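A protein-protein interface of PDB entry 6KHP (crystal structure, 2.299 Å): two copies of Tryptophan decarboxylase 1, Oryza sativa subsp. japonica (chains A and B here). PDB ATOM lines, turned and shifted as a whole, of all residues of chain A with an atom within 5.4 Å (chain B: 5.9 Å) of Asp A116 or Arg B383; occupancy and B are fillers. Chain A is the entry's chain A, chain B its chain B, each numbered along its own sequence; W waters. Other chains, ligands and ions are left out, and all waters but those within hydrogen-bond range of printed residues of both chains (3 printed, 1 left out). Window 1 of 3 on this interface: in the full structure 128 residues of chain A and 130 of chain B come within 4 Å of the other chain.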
ATOM      1  N   ALA A 111       7.238  38.902   3.806  1.00  0.00           N
ATOM      2  CA  ALA A 111       6.182  38.274   3.014  1.00  0.00           C
ATOM      3  C   ALA A 111       5.969  36.814   3.415  1.00  0.00           C
ATOM      4  O   ALA A 111       4.827  36.368   3.573  1.00  0.00           O
ATOM      5  CB  ALA A 111       6.495  38.390   1.515  1.00  0.00           C
ATOM      6  N   ALA A 112       7.051  36.049   3.587  1.00  0.00           N
ATOM      7  CA  ALA A 112       6.911  34.642   3.974  1.00  0.00           C
ATOM      8  C   ALA A 112       6.275  34.496   5.352  1.00  0.00           C
ATOM      9  O   ALA A 112       5.393  33.651   5.555  1.00  0.00           O
ATOM     10  CB  ALA A 112       8.273  33.952   3.955  1.00  0.00           C
ATOM     11  N   ILE A 113       6.718  35.303   6.315  1.00  0.00           N
ATOM     12  CA  ILE A 113       6.112  35.273   7.642  1.00  0.00           C
ATOM     13  C   ILE A 113       4.627  35.623   7.556  1.00  0.00           C
ATOM     14  O   ILE A 113       3.786  34.993   8.211  1.00  0.00           O
ATOM     15  CB  ILE A 113       6.872  36.222   8.591  1.00  0.00           C
ATOM     16  CG1 ILE A 113       8.338  35.793   8.712  1.00  0.00           C
ATOM     17  CG2 ILE A 113       6.213  36.276   9.955  1.00  0.00           C
ATOM     18  CD1 ILE A 113       9.214  36.786   9.525  1.00  0.00           C
ATOM     19  N   ALA A 114       4.277  36.618   6.733  1.00  0.00           N
ATOM     20  CA  ALA A 114       2.873  36.997   6.599  1.00  0.00           C
ATOM     21  C   ALA A 114       2.064  35.869   5.978  1.00  0.00           C
ATOM     22  O   ALA A 114       0.958  35.561   6.435  1.00  0.00           O
ATOM     23  CB  ALA A 114       2.747  38.267   5.755  1.00  0.00           C
ATOM     24  N   GLY A 115       2.616  35.235   4.941  1.00  0.00           N
ATOM     25  CA  GLY A 115       1.953  34.096   4.332  1.00  0.00           C
ATOM     26  C   GLY A 115       1.710  32.956   5.304  1.00  0.00           C
ATOM     27  O   GLY A 115       0.606  32.408   5.362  1.00  0.00           O
ATOM     28  N   ASP A 116       2.739  32.569   6.074  1.00  0.00           N
ATOM     29  CA  ASP A 116       2.547  31.476   7.024  1.00  0.00           C
ATOM     30  C   ASP A 116       1.564  31.862   8.121  1.00  0.00           C
ATOM     31  O   ASP A 116       0.786  31.018   8.575  1.00  0.00           O
ATOM     32  CB  ASP A 116       3.882  31.039   7.639  1.00  0.00           C
ATOM     33  CG  ASP A 116       4.297  29.634   7.203  1.00  0.00           C
ATOM     34  OD1 ASP A 116       3.554  28.992   6.418  1.00  0.00           O
ATOM     35  OD2 ASP A 116       5.376  29.172   7.629  1.00  0.00           O
ATOM     36  N   LEU A 117       1.564  33.124   8.540  1.00  0.00           N
ATOM     37  CA  LEU A 117       0.583  33.572   9.529  1.00  0.00           C
ATOM     38  C   LEU A 117      -0.839  33.377   9.015  1.00  0.00           C
ATOM     39  O   LEU A 117      -1.698  32.827   9.712  1.00  0.00           O
ATOM     40  CB  LEU A 117       0.838  35.041   9.899  1.00  0.00           C
ATOM     41  CG  LEU A 117      -0.252  35.781  10.683  1.00  0.00           C
ATOM     42  CD1 LEU A 117      -0.621  35.046  11.978  1.00  0.00           C
ATOM     43  CD2 LEU A 117       0.151  37.228  10.949  1.00  0.00           C
ATOM     44  N   ILE A 118      -1.102  33.803   7.779  1.00  0.00           N
ATOM     45  CA  ILE A 118      -2.444  33.653   7.231  1.00  0.00           C
ATOM     46  C   ILE A 118      -2.801  32.174   7.064  1.00  0.00           C
ATOM     47  O   ILE A 118      -3.934  31.759   7.350  1.00  0.00           O
ATOM     48  CB  ILE A 118      -2.555  34.439   5.914  1.00  0.00           C
ATOM     49  CG1 ILE A 118      -2.418  35.940   6.210  1.00  0.00           C
ATOM     50  CG2 ILE A 118      -3.890  34.140   5.203  1.00  0.00           C
ATOM     51  CD1 ILE A 118      -1.997  36.781   4.997  1.00  0.00           C
ATOM     52  N   ALA A 119      -1.838  31.350   6.630  1.00  0.00           N
ATOM     53  CA  ALA A 119      -2.107  29.923   6.494  1.00  0.00           C
ATOM     54  C   ALA A 119      -2.412  29.300   7.852  1.00  0.00           C
ATOM     55  O   ALA A 119      -3.303  28.451   7.967  1.00  0.00           O
ATOM     56  CB  ALA A 119      -0.923  29.222   5.811  1.00  0.00           C
ATOM     57  N   SER A 120      -1.688  29.716   8.894  1.00  0.00           N
ATOM     58  CA  SER A 120      -1.983  29.244  10.249  1.00  0.00           C
ATOM     59  C   SER A 120      -3.376  29.636  10.689  1.00  0.00           C
ATOM     60  O   SER A 120      -4.010  28.904  11.452  1.00  0.00           O
ATOM     61  CB  SER A 120      -0.978  29.808  11.256  1.00  0.00           C
ATOM     62  OG  SER A 120       0.316  29.270  11.032  1.00  0.00           O
ATOM     63  N   ALA A 121      -3.860  30.802  10.256  1.00  0.00           N
ATOM     64  CA  ALA A 121      -5.177  31.222  10.708  1.00  0.00           C
ATOM     65  C   ALA A 121      -6.279  30.505   9.933  1.00  0.00           C
ATOM     66  O   ALA A 121      -7.254  30.032  10.524  1.00  0.00           O
ATOM     67  CB  ALA A 121      -5.320  32.738  10.584  1.00  0.00           C
ATOM     68  N   CYS A 335      10.361  31.104   5.346  1.00  0.00           N
ATOM     69  CA  CYS A 335      10.585  30.478   6.650  1.00  0.00           C
ATOM     70  C   CYS A 335      10.247  28.985   6.629  1.00  0.00           C
ATOM     71  O   CYS A 335       9.407  28.528   5.845  1.00  0.00           O
ATOM     72  CB  CYS A 335       9.756  31.197   7.735  1.00  0.00           C
ATOM     73  SG  CYS A 335       7.951  31.122   7.512  1.00  0.00           S
ATOM     74  N   LEU A 336      10.922  28.219   7.498  1.00  0.00           N
ATOM     75  CA  LEU A 336      10.653  26.789   7.638  1.00  0.00           C
ATOM     76  C   LEU A 336       9.185  26.553   7.977  1.00  0.00           C
ATOM     77  O   LEU A 336       8.564  27.344   8.697  1.00  0.00           O
ATOM     78  CB  LEU A 336      11.531  26.183   8.740  1.00  0.00           C
ATOM     79  CG  LEU A 336      13.011  25.878   8.473  1.00  0.00           C
ATOM     80  CD1 LEU A 336      13.872  27.140   8.526  1.00  0.00           C
ATOM     81  CD2 LEU A 336      13.542  24.795   9.430  1.00  0.00           C
ATOM     82  N   ASP A 337       8.614  25.451   7.482  1.00  0.00           N
ATOM     83  CA  ASP A 337       9.248  24.459   6.629  1.00  0.00           C
ATOM     84  C   ASP A 337       8.893  24.736   5.173  1.00  0.00           C
ATOM     85  O   ASP A 337       7.771  25.123   4.886  1.00  0.00           O
ATOM     86  CB  ASP A 337       8.792  23.033   6.996  1.00  0.00           C
ATOM     87  CG  ASP A 337       8.853  22.747   8.491  1.00  0.00           C
ATOM     88  OD1 ASP A 337       9.824  23.160   9.152  1.00  0.00           O
ATOM     89  OD2 ASP A 337       7.920  22.086   9.006  1.00  0.00           O
ATOM     90  N   ARG A 383      -0.361  21.455   5.589  1.00  0.00           N
ATOM     91  CA  ARG A 383      -0.607  22.881   5.659  1.00  0.00           C
ATOM     92  C   ARG A 383      -0.665  23.484   4.260  1.00  0.00           C
ATOM     93  O   ARG A 383      -0.197  22.899   3.277  1.00  0.00           O
ATOM     94  CB  ARG A 383       0.520  23.585   6.420  1.00  0.00           C
ATOM     95  CG  ARG A 383       0.422  23.596   7.912  1.00  0.00           C
ATOM     96  CD  ARG A 383       1.710  24.192   8.499  1.00  0.00           C
ATOM     97  NE  ARG A 383       1.888  25.570   8.056  1.00  0.00           N
ATOM     98  CZ  ARG A 383       1.330  26.597   8.663  1.00  0.00           C
ATOM     99  NH1 ARG A 383       0.592  26.385   9.751  1.00  0.00           N
ATOM    100  NH2 ARG A 383       1.520  27.829   8.210  1.00  0.00           N
ATOM    101  N   PHE A 384      -1.167  24.720   4.204  1.00  0.00           N
ATOM    102  CA  PHE A 384      -1.167  25.543   2.992  1.00  0.00           C
ATOM    103  C   PHE A 384       0.195  26.237   2.858  1.00  0.00           C
ATOM    104  O   PHE A 384       0.345  27.449   3.013  1.00  0.00           O
ATOM    105  CB  PHE A 384      -2.331  26.529   3.066  1.00  0.00           C
ATOM    106  CG  PHE A 384      -2.548  27.360   1.825  1.00  0.00           C
ATOM    107  CD1 PHE A 384      -1.846  27.124   0.656  1.00  0.00           C
ATOM    108  CD2 PHE A 384      -3.478  28.397   1.846  1.00  0.00           C
ATOM    109  CE1 PHE A 384      -2.058  27.906  -0.461  1.00  0.00           C
ATOM    110  CE2 PHE A 384      -3.695  29.171   0.743  1.00  0.00           C
ATOM    111  CZ  PHE A 384      -2.979  28.936  -0.420  1.00  0.00           C
ATOM    112  N   ARG A 385       1.214  25.433   2.537  1.00  0.00           N
ATOM    113  CA  ARG A 385       2.568  25.972   2.462  1.00  0.00           C
ATOM    114  C   ARG A 385       2.827  26.716   1.164  1.00  0.00           C
ATOM    115  O   ARG A 385       3.768  27.520   1.104  1.00  0.00           O
ATOM    116  CB  ARG A 385       3.602  24.854   2.646  1.00  0.00           C
ATOM    117  CG  ARG A 385       3.769  24.441   4.109  1.00  0.00           C
ATOM    118  CD  ARG A 385       5.110  23.759   4.407  1.00  0.00           C
ATOM    119  NE  ARG A 385       4.922  22.325   4.504  1.00  0.00           N
ATOM    120  CZ  ARG A 385       4.700  21.650   5.632  1.00  0.00           C
ATOM    121  NH1 ARG A 385       4.679  22.262   6.833  1.00  0.00           N
ATOM    122  NH2 ARG A 385       4.532  20.329   5.549  1.00  0.00           N
ATOM    123  N   LYS A 388       2.948  31.049   1.474  1.00  0.00           N
ATOM    124  CA  LYS A 388       4.149  31.827   1.782  1.00  0.00           C
ATOM    125  C   LYS A 388       5.097  31.875   0.596  1.00  0.00           C
ATOM    126  O   LYS A 388       5.620  32.947   0.259  1.00  0.00           O
ATOM    127  CB  LYS A 388       4.873  31.283   3.019  1.00  0.00           C
ATOM    128  CG  LYS A 388       5.406  29.858   2.944  1.00  0.00           C
ATOM    129  CD  LYS A 388       6.063  29.515   4.284  1.00  0.00           C
ATOM    130  CE  LYS A 388       6.207  28.015   4.465  1.00  0.00           C
ATOM    131  NZ  LYS A 388       6.674  27.624   5.842  1.00  0.00           N
ATOM    132  N   GLY B 115       1.852  31.843  18.676  1.00  0.00           N
ATOM    133  CA  GLY B 115       3.075  31.077  18.868  1.00  0.00           C
ATOM    134  C   GLY B 115       3.725  30.641  17.563  1.00  0.00           C
ATOM    135  O   GLY B 115       4.955  30.668  17.426  1.00  0.00           O
ATOM    136  N   ASP B 116       2.915  30.234  16.577  1.00  0.00           N
ATOM    137  CA  ASP B 116       3.505  29.856  15.297  1.00  0.00           C
ATOM    138  C   ASP B 116       4.003  31.068  14.532  1.00  0.00           C
ATOM    139  O   ASP B 116       5.005  30.972  13.815  1.00  0.00           O
ATOM    140  CB  ASP B 116       2.514  29.058  14.456  1.00  0.00           C
ATOM    141  CG  ASP B 116       2.946  27.618  14.281  1.00  0.00           C
ATOM    142  OD1 ASP B 116       3.946  27.213  14.928  1.00  0.00           O
ATOM    143  OD2 ASP B 116       2.284  26.896  13.509  1.00  0.00           O
ATOM    144  N   LEU B 117       3.320  32.209  14.670  1.00  0.00           N
ATOM    145  CA  LEU B 117       3.839  33.453  14.115  1.00  0.00           C
ATOM    146  C   LEU B 117       5.219  33.765  14.685  1.00  0.00           C
ATOM    147  O   LEU B 117       6.155  34.071  13.942  1.00  0.00           O
ATOM    148  CB  LEU B 117       2.860  34.590  14.407  1.00  0.00           C
ATOM    149  CG  LEU B 117       3.385  36.007  14.180  1.00  0.00           C
ATOM    150  CD1 LEU B 117       3.904  36.179  12.750  1.00  0.00           C
ATOM    151  CD2 LEU B 117       2.288  37.037  14.489  1.00  0.00           C
ATOM    152  N   ALA B 119       7.348  31.703  16.160  1.00  0.00           N
ATOM    153  CA  ALA B 119       8.332  30.716  15.700  1.00  0.00           C
ATOM    154  C   ALA B 119       8.770  30.998  14.263  1.00  0.00           C
ATOM    155  O   ALA B 119       9.955  30.843  13.926  1.00  0.00           O
ATOM    156  CB  ALA B 119       7.765  29.301  15.825  1.00  0.00           C
ATOM    157  N   SER B 120       7.832  31.421  13.403  1.00  0.00           N
ATOM    158  CA  SER B 120       8.176  31.721  12.014  1.00  0.00           C
ATOM    159  C   SER B 120       9.167  32.864  11.923  1.00  0.00           C
ATOM    160  O   SER B 120       9.987  32.899  11.000  1.00  0.00           O
ATOM    161  CB  SER B 120       6.924  32.076  11.211  1.00  0.00           C
ATOM    162  OG  SER B 120       6.105  30.929  11.036  1.00  0.00           O
ATOM    163  N   ASN B 123      12.528  31.654  13.502  1.00  0.00           N
ATOM    164  CA  ASN B 123      12.958  30.788  12.403  1.00  0.00           C
ATOM    165  C   ASN B 123      14.228  30.004  12.736  1.00  0.00           C
ATOM    166  O   ASN B 123      15.180  29.954  11.951  1.00  0.00           O
ATOM    167  CB  ASN B 123      13.144  31.602  11.126  1.00  0.00           C
ATOM    168  CG  ASN B 123      12.982  30.758   9.890  1.00  0.00           C
ATOM    169  OD1 ASN B 123      12.155  29.842   9.850  1.00  0.00           O
ATOM    170  ND2 ASN B 123      13.781  31.044   8.879  1.00  0.00           N
ATOM    171  N   THR B 124      14.231  29.371  13.905  1.00  0.00           N
ATOM    172  CA  THR B 124      15.353  28.540  14.318  1.00  0.00           C
ATOM    173  C   THR B 124      15.140  27.109  13.849  1.00  0.00           C
ATOM    174  O   THR B 124      14.008  26.664  13.638  1.00  0.00           O
ATOM    175  CB  THR B 124      15.528  28.566  15.841  1.00  0.00           C
ATOM    176  OG1 THR B 124      14.351  28.044  16.466  1.00  0.00           O
ATOM    177  CG2 THR B 124      15.765  29.999  16.337  1.00  0.00           C
ATOM    178  N   VAL B 125      16.256  26.400  13.664  1.00  0.00           N
ATOM    179  CA  VAL B 125      16.275  24.999  13.258  1.00  0.00           C
ATOM    180  C   VAL B 125      16.883  24.215  14.409  1.00  0.00           C
ATOM    181  O   VAL B 125      18.071  24.374  14.710  1.00  0.00           O
ATOM    182  CB  VAL B 125      17.079  24.784  11.970  1.00  0.00           C
ATOM    183  CG1 VAL B 125      16.713  23.457  11.342  1.00  0.00           C
ATOM    184  CG2 VAL B 125      16.858  25.952  10.993  1.00  0.00           C
ATOM    185  N   GLY B 126      16.087  23.363  15.045  1.00  0.00           N
ATOM    186  CA  GLY B 126      16.530  22.739  16.275  1.00  0.00           C
ATOM    187  C   GLY B 126      16.977  21.299  16.131  1.00  0.00           C
ATOM    188  O   GLY B 126      16.521  20.434  16.886  1.00  0.00           O
ATOM    189  N   GLU B 139      10.044  21.919  23.564  1.00  0.00           N
ATOM    190  CA  GLU B 139       9.356  20.765  22.989  1.00  0.00           C
ATOM    191  C   GLU B 139       9.242  19.643  24.008  1.00  0.00           C
ATOM    192  O   GLU B 139       8.186  19.015  24.136  1.00  0.00           O
ATOM    193  CB  GLU B 139      10.071  20.278  21.717  1.00  0.00           C
ATOM    194  CG  GLU B 139      10.126  21.351  20.624  1.00  0.00           C
ATOM    195  CD  GLU B 139       9.825  20.830  19.216  1.00  0.00           C
ATOM    196  OE1 GLU B 139       9.537  21.690  18.351  1.00  0.00           O
ATOM    197  OE2 GLU B 139       9.885  19.592  18.974  1.00  0.00           O
ATOM    198  N   GLY B 381      15.735  18.631  11.587  1.00  0.00           N
ATOM    199  CA  GLY B 381      15.923  19.857  10.846  1.00  0.00           C
ATOM    200  C   GLY B 381      14.597  20.447  10.406  1.00  0.00           C
ATOM    201  O   GLY B 381      14.339  20.568   9.201  1.00  0.00           O
ATOM    202  N   ARG B 382      13.749  20.811  11.372  1.00  0.00           N
ATOM    203  CA  ARG B 382      12.471  21.448  11.076  1.00  0.00           C
ATOM    204  C   ARG B 382      12.155  22.469  12.174  1.00  0.00           C
ATOM    205  O   ARG B 382      12.907  22.631  13.146  1.00  0.00           O
ATOM    206  CB  ARG B 382      11.357  20.401  10.894  1.00  0.00           C
ATOM    207  CG  ARG B 382      11.330  19.296  11.958  1.00  0.00           C
ATOM    208  CD  ARG B 382      10.871  19.819  13.315  1.00  0.00           C
ATOM    209  NE  ARG B 382      10.845  18.776  14.334  1.00  0.00           N
ATOM    210  CZ  ARG B 382      10.450  18.958  15.592  1.00  0.00           C
ATOM    211  NH1 ARG B 382      10.036  20.157  16.004  1.00  0.00           N
ATOM    212  NH2 ARG B 382      10.474  17.940  16.438  1.00  0.00           N
ATOM    213  N   ARG B 383      11.017  23.147  12.020  1.00  0.00           N
ATOM    214  CA  ARG B 383      10.753  24.359  12.786  1.00  0.00           C
ATOM    215  C   ARG B 383      10.391  24.054  14.235  1.00  0.00           C
ATOM    216  O   ARG B 383      10.167  22.913  14.642  1.00  0.00           O
ATOM    217  CB  ARG B 383       9.635  25.177  12.147  1.00  0.00           C
ATOM    218  CG  ARG B 383       8.331  24.424  11.926  1.00  0.00           C
ATOM    219  CD  ARG B 383       7.380  25.308  11.148  1.00  0.00           C
ATOM    220  NE  ARG B 383       6.742  26.264  12.039  1.00  0.00           N
ATOM    221  CZ  ARG B 383       6.459  27.523  11.732  1.00  0.00           C
ATOM    222  NH1 ARG B 383       6.753  28.010  10.529  1.00  0.00           N
ATOM    223  NH2 ARG B 383       5.856  28.291  12.634  1.00  0.00           N
ATOM    224  N   PHE B 384      10.327  25.132  15.007  1.00  0.00           N
ATOM    225  CA  PHE B 384      10.046  25.132  16.440  1.00  0.00           C
ATOM    226  C   PHE B 384       8.543  24.924  16.652  1.00  0.00           C
ATOM    227  O   PHE B 384       7.786  25.851  16.953  1.00  0.00           O
ATOM    228  CB  PHE B 384      10.544  26.452  17.022  1.00  0.00           C
ATOM    229  CG  PHE B 384      10.431  26.576  18.507  1.00  0.00           C
ATOM    230  CD1 PHE B 384      10.062  25.498  19.311  1.00  0.00           C
ATOM    231  CD2 PHE B 384      10.725  27.790  19.107  1.00  0.00           C
ATOM    232  CE1 PHE B 384       9.975  25.638  20.689  1.00  0.00           C
ATOM    233  CE2 PHE B 384      10.643  27.945  20.483  1.00  0.00           C
ATOM    234  CZ  PHE B 384      10.265  26.865  21.280  1.00  0.00           C
ATOM    235  N   ARG B 385       8.110  23.667  16.530  1.00  0.00           N
ATOM    236  CA  ARG B 385       6.692  23.360  16.718  1.00  0.00           C
ATOM    237  C   ARG B 385       6.240  23.457  18.177  1.00  0.00           C
ATOM    238  O   ARG B 385       5.032  23.535  18.435  1.00  0.00           O
ATOM    239  CB  ARG B 385       6.384  21.959  16.174  1.00  0.00           C
ATOM    240  CG  ARG B 385       6.547  21.825  14.648  1.00  0.00           C
ATOM    241  CD  ARG B 385       6.698  20.355  14.287  1.00  0.00           C
ATOM    242  NE  ARG B 385       6.833  20.099  12.865  1.00  0.00           N
ATOM    243  CZ  ARG B 385       7.335  18.966  12.364  1.00  0.00           C
ATOM    244  NH1 ARG B 385       7.755  17.998  13.185  1.00  0.00           N
ATOM    245  NH2 ARG B 385       7.424  18.797  11.048  1.00  0.00           N
ATOM    246  N   GLY B 386       7.166  23.443  19.143  1.00  0.00           N
ATOM    247  CA  GLY B 386       6.757  23.353  20.535  1.00  0.00           C
ATOM    248  C   GLY B 386       6.193  24.638  21.110  1.00  0.00           C
ATOM    249  O   GLY B 386       5.396  24.599  22.058  1.00  0.00           O
ATOM    250  N   LYS B 388       4.026  26.912  20.121  1.00  0.00           N
ATOM    251  CA  LYS B 388       2.584  27.141  20.071  1.00  0.00           C
ATOM    252  C   LYS B 388       1.831  26.184  20.990  1.00  0.00           C
ATOM    253  O   LYS B 388       0.784  26.550  21.536  1.00  0.00           O
ATOM    254  CB  LYS B 388       2.070  27.002  18.635  1.00  0.00           C
ATOM    255  CG  LYS B 388       2.196  25.589  18.108  1.00  0.00           C
ATOM    256  CD  LYS B 388       1.907  25.488  16.635  1.00  0.00           C
ATOM    257  CE  LYS B 388       2.554  24.228  16.065  1.00  0.00           C
ATOM    258  NZ  LYS B 388       2.203  24.016  14.633  1.00  0.00           N
HETATM  259  O   HOH W   1       2.989  30.908  11.302  1.00  0.00           O
HETATM  260  O   HOH W   2       5.884  21.621  10.859  1.00  0.00           O
HETATM  261  O   HOH W   3       4.091  33.144  10.406  1.00  0.00           O
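The side-chain carboxylate (OD2) of Asp A116 is in salt-bridge range of the guanidinium group (NH1) of Arg B383, 3.4 Å away.
The backbone NH of Leu A336 is in hydrogen-bond range of the side-chain amide oxygen of Asn B123 (3.1 Å).
The backbone carbonyl oxygen (O) of Leu A336 lies within hydrogen-bond range of the guanidinium group (NH1) of Arg B383.
OD1 of Asp A337 lies within hydrogen-bond range of N of Arg B383 (3.1 Å).
OD2 of Asp A337 lies within salt-bridge range of NH2 of Arg B385, 3.9 Å away.
OG of Ser A120 is in hydrogen-bond range of O of Asp A116, at 3.1 Å.
The side-chain carboxylate of Asp A116 is in salt-bridge range of the side-chain amino group of Lys A388.
The backbone carbonyl oxygen (O) of Leu A336 sits at hydrogen-bond distance from the side-chain amino group (NZ) of Lys A388 (3.4 Å).
The side-chain carboxylate (OD2) of Asp A337 lies within salt-bridge range of the guanidinium group (NH1) of Arg A385 (3.9 Å).
The side-chain amino group (NZ) of Lys A388 lies within hydrogen-bond range of the backbone carbonyl oxygen (O) of Asp A337.
The side-chain hydroxyl (OG) of Ser B120 is in hydrogen-bond range of the backbone carbonyl oxygen (O) of Asp B116 (3.0 Å).
Among the printed residues, pairs that only touch across the chains: Cys A335 with Asn B123, Asp A337 with Arg B382, Ile A113 with Leu B117, Cys A335 with Ser B120, Leu A336 with Val B125, Leu A336 with Arg B382, Asp A116 with Ser B120 and Ser A120 with Asp B116.
Of chain B, only Ser B120 and Arg B383 come within 4 Å of Asp A116.
Of the printed residues of chain A, Ser B120 touches Asp A116 (3.9 Å) and Cys A335 (3.7 Å).
Of the printed residues of chain A, Asn B123 touches Cys A335 (3.5 Å) and Leu A336 (3.1 Å).
Glu B139 touches none of the printed residues of chain A.
Of the printed residues of chain A, Arg B382 touches Leu A336 (3.9 Å) and Asp A337 (3.6 Å).
Of chain A, only Asp A116 (3.4 Å), Leu A336 (2.7 Å) and Asp A337 (3.1 Å) come within 4 Å of Arg B383.
Gly B386 touches none of the printed residues of chain A.
The nearest printed residue of chain B that does not touch Asp A116 is Asp B116 (6.3 Å).
Of the 18 printed residues of chain A, 6 touch a printed residue of chain B.
Printed residues of chain A that touch a printed residue of chain B: Ile A113, Asp A116, Ser A120, Cys A335, Leu A336 and Asp A337.
Hydrophobic or aromatic side chains of chain A that line the printed part of chain B: Ile A113 and Leu A336.
Of the 17 printed residues of chain B, 8 touch a printed residue of chain A.
Hydrophobic or aromatic side chains of chain B within 4 Å of the printed part of chain A: Leu B117 and Val B125.
Among the printed residues, Asp or Glu carboxylates within 4 Å of a Lys or Arg side-chain nitrogen of the other chain: Asp A116 with Arg B383 and Asp A337 with Arg B385.
Asp A116 touches Ser B120, and with the chains exchanged Ser A120 touches Asp B116.
Asp A116 touches Arg B383, but with the chains exchanged Arg A383 does not touch Asp B116 (4.2 Å).
Positions printed for both chains: 115, 116, 117, 119, 120, 383, 384, 385 and 388.
Of the 13 pairs that touch across the chains among the printed residues, 2 have their exchanged pair printed and touching as well.
Water W2 bridges the guanidinium group (NE) of Arg B385 (2.7 Å) and the side-chain carboxylate (OD2) of Asp A337 (2.8 Å).
Water W3 lies within hydrogen-bond range of O of Ile A113 (2.9 Å), OG of Ser B120 (3.1 Å) and N of Leu A117 (3.1 Å).
Water W1 lies within hydrogen-bond range of the side-chain hydroxyl of Ser B120 (3.1 Å), the side-chain hydroxyl of Ser A120 (3.1 Å) and the backbone carbonyl oxygen of Asp B116 (3.2 Å).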
